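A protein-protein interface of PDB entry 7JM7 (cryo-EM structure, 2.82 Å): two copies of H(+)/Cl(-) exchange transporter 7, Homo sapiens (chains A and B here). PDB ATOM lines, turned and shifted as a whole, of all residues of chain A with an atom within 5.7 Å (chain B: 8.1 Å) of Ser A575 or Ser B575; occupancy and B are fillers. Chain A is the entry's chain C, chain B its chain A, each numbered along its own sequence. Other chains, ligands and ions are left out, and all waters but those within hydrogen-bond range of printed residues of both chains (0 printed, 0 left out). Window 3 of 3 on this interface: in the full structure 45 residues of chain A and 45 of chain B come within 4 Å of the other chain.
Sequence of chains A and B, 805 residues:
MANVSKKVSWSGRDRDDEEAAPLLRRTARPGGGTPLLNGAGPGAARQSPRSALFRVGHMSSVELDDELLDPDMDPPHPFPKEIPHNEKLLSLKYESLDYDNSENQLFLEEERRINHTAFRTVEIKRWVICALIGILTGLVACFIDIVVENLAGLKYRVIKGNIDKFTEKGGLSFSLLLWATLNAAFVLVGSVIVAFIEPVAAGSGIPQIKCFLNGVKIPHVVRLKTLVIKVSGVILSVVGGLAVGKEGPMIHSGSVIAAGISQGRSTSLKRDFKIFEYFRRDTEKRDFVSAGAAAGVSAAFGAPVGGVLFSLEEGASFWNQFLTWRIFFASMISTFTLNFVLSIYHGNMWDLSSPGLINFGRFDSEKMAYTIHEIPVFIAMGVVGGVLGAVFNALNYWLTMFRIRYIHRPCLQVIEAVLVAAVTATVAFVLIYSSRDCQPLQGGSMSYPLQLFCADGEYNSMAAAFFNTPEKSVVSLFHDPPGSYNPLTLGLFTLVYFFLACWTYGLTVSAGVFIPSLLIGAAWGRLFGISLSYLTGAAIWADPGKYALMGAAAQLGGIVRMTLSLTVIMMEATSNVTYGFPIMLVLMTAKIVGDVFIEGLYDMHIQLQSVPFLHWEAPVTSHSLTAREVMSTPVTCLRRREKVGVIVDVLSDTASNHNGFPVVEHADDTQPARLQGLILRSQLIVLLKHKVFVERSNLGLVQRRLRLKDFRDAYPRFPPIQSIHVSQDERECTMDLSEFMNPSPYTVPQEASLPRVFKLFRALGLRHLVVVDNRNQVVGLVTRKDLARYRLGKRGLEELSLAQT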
ATOM      1  N   GLY A 361     -28.574 -19.856  18.005  1.00  0.00           N
ATOM      2  CA  GLY A 361     -27.273 -19.623  17.427  1.00  0.00           C
ATOM      3  C   GLY A 361     -27.282 -18.466  16.449  1.00  0.00           C
ATOM      4  O   GLY A 361     -28.214 -17.659  16.393  1.00  0.00           O
ATOM      5  N   ARG A 362     -26.214 -18.391  15.661  1.00  0.00           N
ATOM      6  CA  ARG A 362     -26.032 -17.333  14.677  1.00  0.00           C
ATOM      7  C   ARG A 362     -26.282 -17.885  13.281  1.00  0.00           C
ATOM      8  O   ARG A 362     -25.655 -18.869  12.876  1.00  0.00           O
ATOM      9  CB  ARG A 362     -24.625 -16.739  14.767  1.00  0.00           C
ATOM     10  CG  ARG A 362     -24.267 -16.195  16.142  1.00  0.00           C
ATOM     11  CD  ARG A 362     -25.086 -14.960  16.501  1.00  0.00           C
ATOM     12  NE  ARG A 362     -24.735 -13.804  15.676  1.00  0.00           N
ATOM     13  CZ  ARG A 362     -25.447 -13.356  14.643  1.00  0.00           C
ATOM     14  NH1 ARG A 362     -26.571 -13.957  14.275  1.00  0.00           N
ATOM     15  NH2 ARG A 362     -25.027 -12.294  13.969  1.00  0.00           N
ATOM     16  N   MET A 570     -38.998 -15.512  16.738  1.00  0.00           N
ATOM     17  CA  MET A 570     -38.093 -16.258  15.871  1.00  0.00           C
ATOM     18  C   MET A 570     -37.078 -15.335  15.211  1.00  0.00           C
ATOM     19  O   MET A 570     -35.910 -15.704  15.055  1.00  0.00           O
ATOM     20  CB  MET A 570     -38.886 -17.027  14.818  1.00  0.00           C
ATOM     21  CG  MET A 570     -39.692 -18.179  15.386  1.00  0.00           C
ATOM     22  SD  MET A 570     -38.666 -19.540  15.970  1.00  0.00           S
ATOM     23  CE  MET A 570     -38.304 -20.380  14.433  1.00  0.00           C
ATOM     24  N   MET A 571     -37.500 -14.134  14.813  1.00  0.00           N
ATOM     25  CA  MET A 571     -36.562 -13.190  14.216  1.00  0.00           C
ATOM     26  C   MET A 571     -35.472 -12.795  15.205  1.00  0.00           C
ATOM     27  O   MET A 571     -34.286 -12.777  14.858  1.00  0.00           O
ATOM     28  CB  MET A 571     -37.307 -11.951  13.724  1.00  0.00           C
ATOM     29  CG  MET A 571     -38.073 -12.164  12.433  1.00  0.00           C
ATOM     30  SD  MET A 571     -39.494 -11.069  12.285  1.00  0.00           S
ATOM     31  CE  MET A 571     -38.682  -9.528  11.892  1.00  0.00           C
ATOM     32  N   GLU A 572     -35.855 -12.470  16.441  1.00  0.00           N
ATOM     33  CA  GLU A 572     -34.865 -12.076  17.440  1.00  0.00           C
ATOM     34  C   GLU A 572     -33.933 -13.229  17.785  1.00  0.00           C
ATOM     35  O   GLU A 572     -32.715 -13.038  17.892  1.00  0.00           O
ATOM     36  CB  GLU A 572     -35.557 -11.563  18.701  1.00  0.00           C
ATOM     37  CG  GLU A 572     -36.438 -10.352  18.486  1.00  0.00           C
ATOM     38  CD  GLU A 572     -36.416  -9.404  19.664  1.00  0.00           C
ATOM     39  OE1 GLU A 572     -35.325  -9.164  20.222  1.00  0.00           O
ATOM     40  OE2 GLU A 572     -37.494  -8.902  20.041  1.00  0.00           O
ATOM     41  N   ALA A 573     -34.481 -14.431  17.973  1.00  0.00           N
ATOM     42  CA  ALA A 573     -33.641 -15.577  18.302  1.00  0.00           C
ATOM     43  C   ALA A 573     -32.682 -15.896  17.163  1.00  0.00           C
ATOM     44  O   ALA A 573     -31.501 -16.179  17.392  1.00  0.00           O
ATOM     45  CB  ALA A 573     -34.515 -16.786  18.626  1.00  0.00           C
ATOM     46  N   THR A 574     -33.178 -15.859  15.926  1.00  0.00           N
ATOM     47  CA  THR A 574     -32.328 -16.027  14.757  1.00  0.00           C
ATOM     48  C   THR A 574     -31.366 -14.861  14.573  1.00  0.00           C
ATOM     49  O   THR A 574     -30.327 -15.025  13.926  1.00  0.00           O
ATOM     50  CB  THR A 574     -33.200 -16.189  13.511  1.00  0.00           C
ATOM     51  OG1 THR A 574     -33.943 -17.411  13.599  1.00  0.00           O
ATOM     52  CG2 THR A 574     -32.361 -16.200  12.255  1.00  0.00           C
ATOM     53  N   SER A 575     -31.690 -13.694  15.127  1.00  0.00           N
ATOM     54  CA  SER A 575     -30.857 -12.498  15.034  1.00  0.00           C
ATOM     55  C   SER A 575     -30.723 -11.998  13.600  1.00  0.00           C
ATOM     56  O   SER A 575     -29.801 -11.236  13.290  1.00  0.00           O
ATOM     57  CB  SER A 575     -29.471 -12.744  15.636  1.00  0.00           C
ATOM     58  OG  SER A 575     -28.704 -11.553  15.646  1.00  0.00           O
ATOM     59  N   ASN A 576     -31.627 -12.414  12.716  1.00  0.00           N
ATOM     60  CA  ASN A 576     -31.647 -11.960  11.332  1.00  0.00           C
ATOM     61  C   ASN A 576     -33.037 -11.439  11.006  1.00  0.00           C
ATOM     62  O   ASN A 576     -34.037 -12.101  11.298  1.00  0.00           O
ATOM     63  CB  ASN A 576     -31.268 -13.086  10.367  1.00  0.00           C
ATOM     64  CG  ASN A 576     -30.989 -12.583   8.967  1.00  0.00           C
ATOM     65  OD1 ASN A 576     -31.678 -11.696   8.464  1.00  0.00           O
ATOM     66  ND2 ASN A 576     -29.972 -13.145   8.330  1.00  0.00           N
ATOM     67  N   VAL A 577     -33.094 -10.254  10.398  1.00  0.00           N
ATOM     68  CA  VAL A 577     -34.380  -9.661  10.055  1.00  0.00           C
ATOM     69  C   VAL A 577     -34.906 -10.213   8.735  1.00  0.00           C
ATOM     70  O   VAL A 577     -36.123 -10.300   8.537  1.00  0.00           O
ATOM     71  CB  VAL A 577     -34.254  -8.129  10.009  1.00  0.00           C
ATOM     72  CG1 VAL A 577     -35.571  -7.489   9.606  1.00  0.00           C
ATOM     73  CG2 VAL A 577     -33.786  -7.593  11.354  1.00  0.00           C
ATOM     74  N   GLY B 302     -34.957  -0.530   7.109  1.00  0.00           N
ATOM     75  CA  GLY B 302     -34.958  -1.982   7.199  1.00  0.00           C
ATOM     76  C   GLY B 302     -35.479  -2.482   8.528  1.00  0.00           C
ATOM     77  O   GLY B 302     -34.951  -3.458   9.074  1.00  0.00           O
ATOM     78  N   PHE B 360     -26.564   0.740   8.653  1.00  0.00           N
ATOM     79  CA  PHE B 360     -25.500   1.095   9.585  1.00  0.00           C
ATOM     80  C   PHE B 360     -24.337   0.118   9.508  1.00  0.00           C
ATOM     81  O   PHE B 360     -23.199   0.488   9.817  1.00  0.00           O
ATOM     82  CB  PHE B 360     -26.071   1.141  11.003  1.00  0.00           C
ATOM     83  CG  PHE B 360     -27.040   2.274  11.239  1.00  0.00           C
ATOM     84  CD1 PHE B 360     -27.467   3.080  10.197  1.00  0.00           C
ATOM     85  CD2 PHE B 360     -27.553   2.504  12.503  1.00  0.00           C
ATOM     86  CE1 PHE B 360     -28.359   4.106  10.415  1.00  0.00           C
ATOM     87  CE2 PHE B 360     -28.450   3.529  12.725  1.00  0.00           C
ATOM     88  CZ  PHE B 360     -28.853   4.329  11.679  1.00  0.00           C
ATOM     89  N   GLY B 361     -24.598  -1.115   9.103  1.00  0.00           N
ATOM     90  CA  GLY B 361     -23.591  -2.146   9.020  1.00  0.00           C
ATOM     91  C   GLY B 361     -23.797  -3.230  10.057  1.00  0.00           C
ATOM     92  O   GLY B 361     -24.854  -3.351  10.682  1.00  0.00           O
ATOM     93  N   ARG B 362     -22.754  -4.035  10.242  1.00  0.00           N
ATOM     94  CA  ARG B 362     -22.774  -5.150  11.176  1.00  0.00           C
ATOM     95  C   ARG B 362     -21.958  -4.796  12.411  1.00  0.00           C
ATOM     96  O   ARG B 362     -20.782  -4.435  12.302  1.00  0.00           O
ATOM     97  CB  ARG B 362     -22.222  -6.420  10.524  1.00  0.00           C
ATOM     98  CG  ARG B 362     -22.951  -6.833   9.254  1.00  0.00           C
ATOM     99  CD  ARG B 362     -24.377  -7.292   9.537  1.00  0.00           C
ATOM    100  NE  ARG B 362     -24.416  -8.558  10.269  1.00  0.00           N
ATOM    101  CZ  ARG B 362     -24.656  -8.681  11.573  1.00  0.00           C
ATOM    102  NH1 ARG B 362     -24.883  -7.613  12.331  1.00  0.00           N
ATOM    103  NH2 ARG B 362     -24.667  -9.884  12.128  1.00  0.00           N
ATOM    104  N   PHE B 363     -22.589  -4.900  13.578  1.00  0.00           N
ATOM    105  CA  PHE B 363     -21.944  -4.631  14.855  1.00  0.00           C
ATOM    106  C   PHE B 363     -21.606  -5.907  15.615  1.00  0.00           C
ATOM    107  O   PHE B 363     -21.269  -5.839  16.802  1.00  0.00           O
ATOM    108  CB  PHE B 363     -22.840  -3.736  15.714  1.00  0.00           C
ATOM    109  CG  PHE B 363     -22.916  -2.314  15.239  1.00  0.00           C
ATOM    110  CD1 PHE B 363     -22.107  -1.341  15.795  1.00  0.00           C
ATOM    111  CD2 PHE B 363     -23.794  -1.951  14.234  1.00  0.00           C
ATOM    112  CE1 PHE B 363     -22.176  -0.032  15.362  1.00  0.00           C
ATOM    113  CE2 PHE B 363     -23.867  -0.645  13.797  1.00  0.00           C
ATOM    114  CZ  PHE B 363     -23.057   0.314  14.362  1.00  0.00           C
ATOM    115  N   ASP B 364     -21.691  -7.065  14.963  1.00  0.00           N
ATOM    116  CA  ASP B 364     -21.401  -8.348  15.601  1.00  0.00           C
ATOM    117  C   ASP B 364     -19.890  -8.516  15.668  1.00  0.00           C
ATOM    118  O   ASP B 364     -19.259  -9.060  14.761  1.00  0.00           O
ATOM    119  CB  ASP B 364     -22.055  -9.490  14.834  1.00  0.00           C
ATOM    120  CG  ASP B 364     -21.721 -10.849  15.415  1.00  0.00           C
ATOM    121  OD1 ASP B 364     -21.387 -10.918  16.617  1.00  0.00           O
ATOM    122  OD2 ASP B 364     -21.793 -11.850  14.671  1.00  0.00           O
ATOM    123  N   VAL B 568     -36.530   0.147  18.734  1.00  0.00           N
ATOM    124  CA  VAL B 568     -36.627  -1.048  17.902  1.00  0.00           C
ATOM    125  C   VAL B 568     -35.968  -0.815  16.548  1.00  0.00           C
ATOM    126  O   VAL B 568     -35.327  -1.714  15.994  1.00  0.00           O
ATOM    127  CB  VAL B 568     -38.096  -1.477  17.753  1.00  0.00           C
ATOM    128  CG1 VAL B 568     -38.201  -2.718  16.887  1.00  0.00           C
ATOM    129  CG2 VAL B 568     -38.709  -1.721  19.115  1.00  0.00           C
ATOM    130  N   ILE B 569     -36.123   0.385  15.988  1.00  0.00           N
ATOM    131  CA  ILE B 569     -35.501   0.697  14.706  1.00  0.00           C
ATOM    132  C   ILE B 569     -33.989   0.595  14.820  1.00  0.00           C
ATOM    133  O   ILE B 569     -33.319   0.003  13.965  1.00  0.00           O
ATOM    134  CB  ILE B 569     -35.938   2.095  14.230  1.00  0.00           C
ATOM    135  CG1 ILE B 569     -37.330   2.028  13.601  1.00  0.00           C
ATOM    136  CG2 ILE B 569     -34.936   2.672  13.243  1.00  0.00           C
ATOM    137  CD1 ILE B 569     -37.985   3.375  13.410  1.00  0.00           C
ATOM    138  N   MET B 570     -33.427   1.180  15.878  1.00  0.00           N
ATOM    139  CA  MET B 570     -31.984   1.113  16.074  1.00  0.00           C
ATOM    140  C   MET B 570     -31.526  -0.319  16.309  1.00  0.00           C
ATOM    141  O   MET B 570     -30.462  -0.719  15.828  1.00  0.00           O
ATOM    142  CB  MET B 570     -31.568   2.010  17.236  1.00  0.00           C
ATOM    143  CG  MET B 570     -31.712   3.491  16.942  1.00  0.00           C
ATOM    144  SD  MET B 570     -30.524   4.091  15.726  1.00  0.00           S
ATOM    145  CE  MET B 570     -29.068   4.299  16.745  1.00  0.00           C
ATOM    146  N   MET B 571     -32.308  -1.106  17.050  1.00  0.00           N
ATOM    147  CA  MET B 571     -31.942  -2.500  17.272  1.00  0.00           C
ATOM    148  C   MET B 571     -31.915  -3.279  15.963  1.00  0.00           C
ATOM    149  O   MET B 571     -30.972  -4.032  15.699  1.00  0.00           O
ATOM    150  CB  MET B 571     -32.917  -3.146  18.255  1.00  0.00           C
ATOM    151  CG  MET B 571     -32.689  -2.751  19.699  1.00  0.00           C
ATOM    152  SD  MET B 571     -34.194  -2.837  20.684  1.00  0.00           S
ATOM    153  CE  MET B 571     -34.353  -4.603  20.888  1.00  0.00           C
ATOM    154  N   GLU B 572     -32.946  -3.115  15.130  1.00  0.00           N
ATOM    155  CA  GLU B 572     -32.988  -3.832  13.859  1.00  0.00           C
ATOM    156  C   GLU B 572     -31.869  -3.386  12.928  1.00  0.00           C
ATOM    157  O   GLU B 572     -31.220  -4.220  12.287  1.00  0.00           O
ATOM    158  CB  GLU B 572     -34.344  -3.637  13.185  1.00  0.00           C
ATOM    159  CG  GLU B 572     -35.524  -4.137  13.987  1.00  0.00           C
ATOM    160  CD  GLU B 572     -36.617  -4.715  13.113  1.00  0.00           C
ATOM    161  OE1 GLU B 572     -36.294  -5.440  12.151  1.00  0.00           O
ATOM    162  OE2 GLU B 572     -37.800  -4.435  13.384  1.00  0.00           O
ATOM    163  N   ALA B 573     -31.632  -2.077  12.833  1.00  0.00           N
ATOM    164  CA  ALA B 573     -30.571  -1.586  11.961  1.00  0.00           C
ATOM    165  C   ALA B 573     -29.208  -2.070  12.435  1.00  0.00           C
ATOM    166  O   ALA B 573     -28.369  -2.483  11.628  1.00  0.00           O
ATOM    167  CB  ALA B 573     -30.612  -0.060  11.902  1.00  0.00           C
ATOM    168  N   THR B 574     -28.970  -2.021  13.746  1.00  0.00           N
ATOM    169  CA  THR B 574     -27.750  -2.568  14.322  1.00  0.00           C
ATOM    170  C   THR B 574     -27.695  -4.085  14.212  1.00  0.00           C
ATOM    171  O   THR B 574     -26.601  -4.658  14.250  1.00  0.00           O
ATOM    172  CB  THR B 574     -27.646  -2.144  15.788  1.00  0.00           C
ATOM    173  OG1 THR B 574     -27.478  -0.723  15.868  1.00  0.00           O
ATOM    174  CG2 THR B 574     -26.482  -2.825  16.471  1.00  0.00           C
ATOM    175  N   SER B 575     -28.845  -4.744  14.079  1.00  0.00           N
ATOM    176  CA  SER B 575     -28.935  -6.195  13.958  1.00  0.00           C
ATOM    177  C   SER B 575     -28.451  -6.911  15.213  1.00  0.00           C
ATOM    178  O   SER B 575     -28.129  -8.102  15.166  1.00  0.00           O
ATOM    179  CB  SER B 575     -28.158  -6.695  12.735  1.00  0.00           C
ATOM    180  OG  SER B 575     -28.337  -8.088  12.555  1.00  0.00           O
ATOM    181  N   ASN B 576     -28.392  -6.205  16.340  1.00  0.00           N
ATOM    182  CA  ASN B 576     -28.009  -6.788  17.618  1.00  0.00           C
ATOM    183  C   ASN B 576     -29.077  -6.462  18.649  1.00  0.00           C
ATOM    184  O   ASN B 576     -29.500  -5.308  18.766  1.00  0.00           O
ATOM    185  CB  ASN B 576     -26.649  -6.262  18.088  1.00  0.00           C
ATOM    186  CG  ASN B 576     -26.087  -7.059  19.246  1.00  0.00           C
ATOM    187  OD1 ASN B 576     -26.816  -7.458  20.153  1.00  0.00           O
ATOM    188  ND2 ASN B 576     -24.783  -7.298  19.219  1.00  0.00           N
ATOM    189  N   VAL B 577     -29.508  -7.479  19.394  1.00  0.00           N
ATOM    190  CA  VAL B 577     -30.541  -7.273  20.400  1.00  0.00           C
ATOM    191  C   VAL B 577     -29.945  -6.747  21.701  1.00  0.00           C
ATOM    192  O   VAL B 577     -30.610  -6.012  22.438  1.00  0.00           O
ATOM    193  CB  VAL B 577     -31.316  -8.582  20.628  1.00  0.00           C
ATOM    194  CG1 VAL B 577     -32.369  -8.403  21.709  1.00  0.00           C
ATOM    195  CG2 VAL B 577     -31.954  -9.055  19.331  1.00  0.00           C
ATOM    196  N   THR B 578     -28.697  -7.110  22.009  1.00  0.00           N
ATOM    197  CA  THR B 578     -28.108  -6.727  23.288  1.00  0.00           C
ATOM    198  C   THR B 578     -27.973  -5.214  23.401  1.00  0.00           C
ATOM    199  O   THR B 578     -28.390  -4.613  24.399  1.00  0.00           O
ATOM    200  CB  THR B 578     -26.746  -7.399  23.459  1.00  0.00           C
ATOM    201  OG1 THR B 578     -25.800  -6.801  22.566  1.00  0.00           O
ATOM    202  CG2 THR B 578     -26.842  -8.888  23.167  1.00  0.00           C
ATOM    203  N   TYR B 579     -27.415  -4.575  22.369  1.00  0.00           N
ATOM    204  CA  TYR B 579     -27.202  -3.133  22.410  1.00  0.00           C
ATOM    205  C   TYR B 579     -28.496  -2.360  22.607  1.00  0.00           C
ATOM    206  O   TYR B 579     -28.446  -1.139  22.794  1.00  0.00           O
ATOM    207  CB  TYR B 579     -26.513  -2.662  21.129  1.00  0.00           C
ATOM    208  CG  TYR B 579     -25.242  -3.410  20.808  1.00  0.00           C
ATOM    209  CD1 TYR B 579     -24.384  -3.825  21.815  1.00  0.00           C
ATOM    210  CD2 TYR B 579     -24.901  -3.703  19.496  1.00  0.00           C
ATOM    211  CE1 TYR B 579     -23.223  -4.514  21.525  1.00  0.00           C
ATOM    212  CE2 TYR B 579     -23.743  -4.389  19.195  1.00  0.00           C
ATOM    213  CZ  TYR B 579     -22.908  -4.792  20.213  1.00  0.00           C
ATOM    214  OH  TYR B 579     -21.755  -5.478  19.919  1.00  0.00           O
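OD2 of Asp B364 lies within salt-bridge range of NH2 of Arg A362 (3.3 Å).
NH2 of Arg B362 lies close to NH2 of Arg A362.
NH1 of Arg A362 sits close to OG of Ser A575, 3.5 Å away.
The guanidinium group (NH1) of Arg B362 sits close to the side-chain hydroxyl (OG) of Ser B575 (3.5 Å).
Among the printed residues, merely in contact across the chains: Val A577 with Glu B572 (3.3 Å), Glu A572 with Val B577 (3.4 Å) and Ser A575 with Ser B575 (3.5 Å).
Of the printed residues of chain B, Arg A362 touches Arg B362 and Asp B364.
Of the printed residues of chain B, Glu A572 touches Val B577.
Of the printed residues of chain B, Ser A575 touches Ser B575.
Of the printed residues of chain B, Val A577 touches Glu B572.
Phe B360 touches none of the printed residues of chain A.
Of the printed residues of chain A, Asp B364 touches Arg A362 (3.3 Å).
The nearest residue of chain B that does not touch Ser A575 is Asn B576 (5.2 Å).
Printed residues of chain A that touch a printed residue of chain B: Arg A362, Glu A572, Ser A575 and Val A577.
Hydrophobic or aromatic side chains of chain A that line the printed part of chain B: Val A577.
Of the 18 printed residues of chain B, 5 touch a printed residue of chain A.
Hydrophobic or aromatic side chains of chain B within 4 Å of the printed part of chain A: Val B577.
Among the printed residues, Asp or Glu carboxylates within 4 Å of a Lys or Arg side-chain nitrogen of the other chain: Arg A362 with Asp B364.
Arg A362 touches its own counterpart, Arg B362.
Glu A572 touches Val B577, and with the chains exchanged Val A577 touches Glu B572.
Ser A575 touches its own counterpart, Ser B575.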
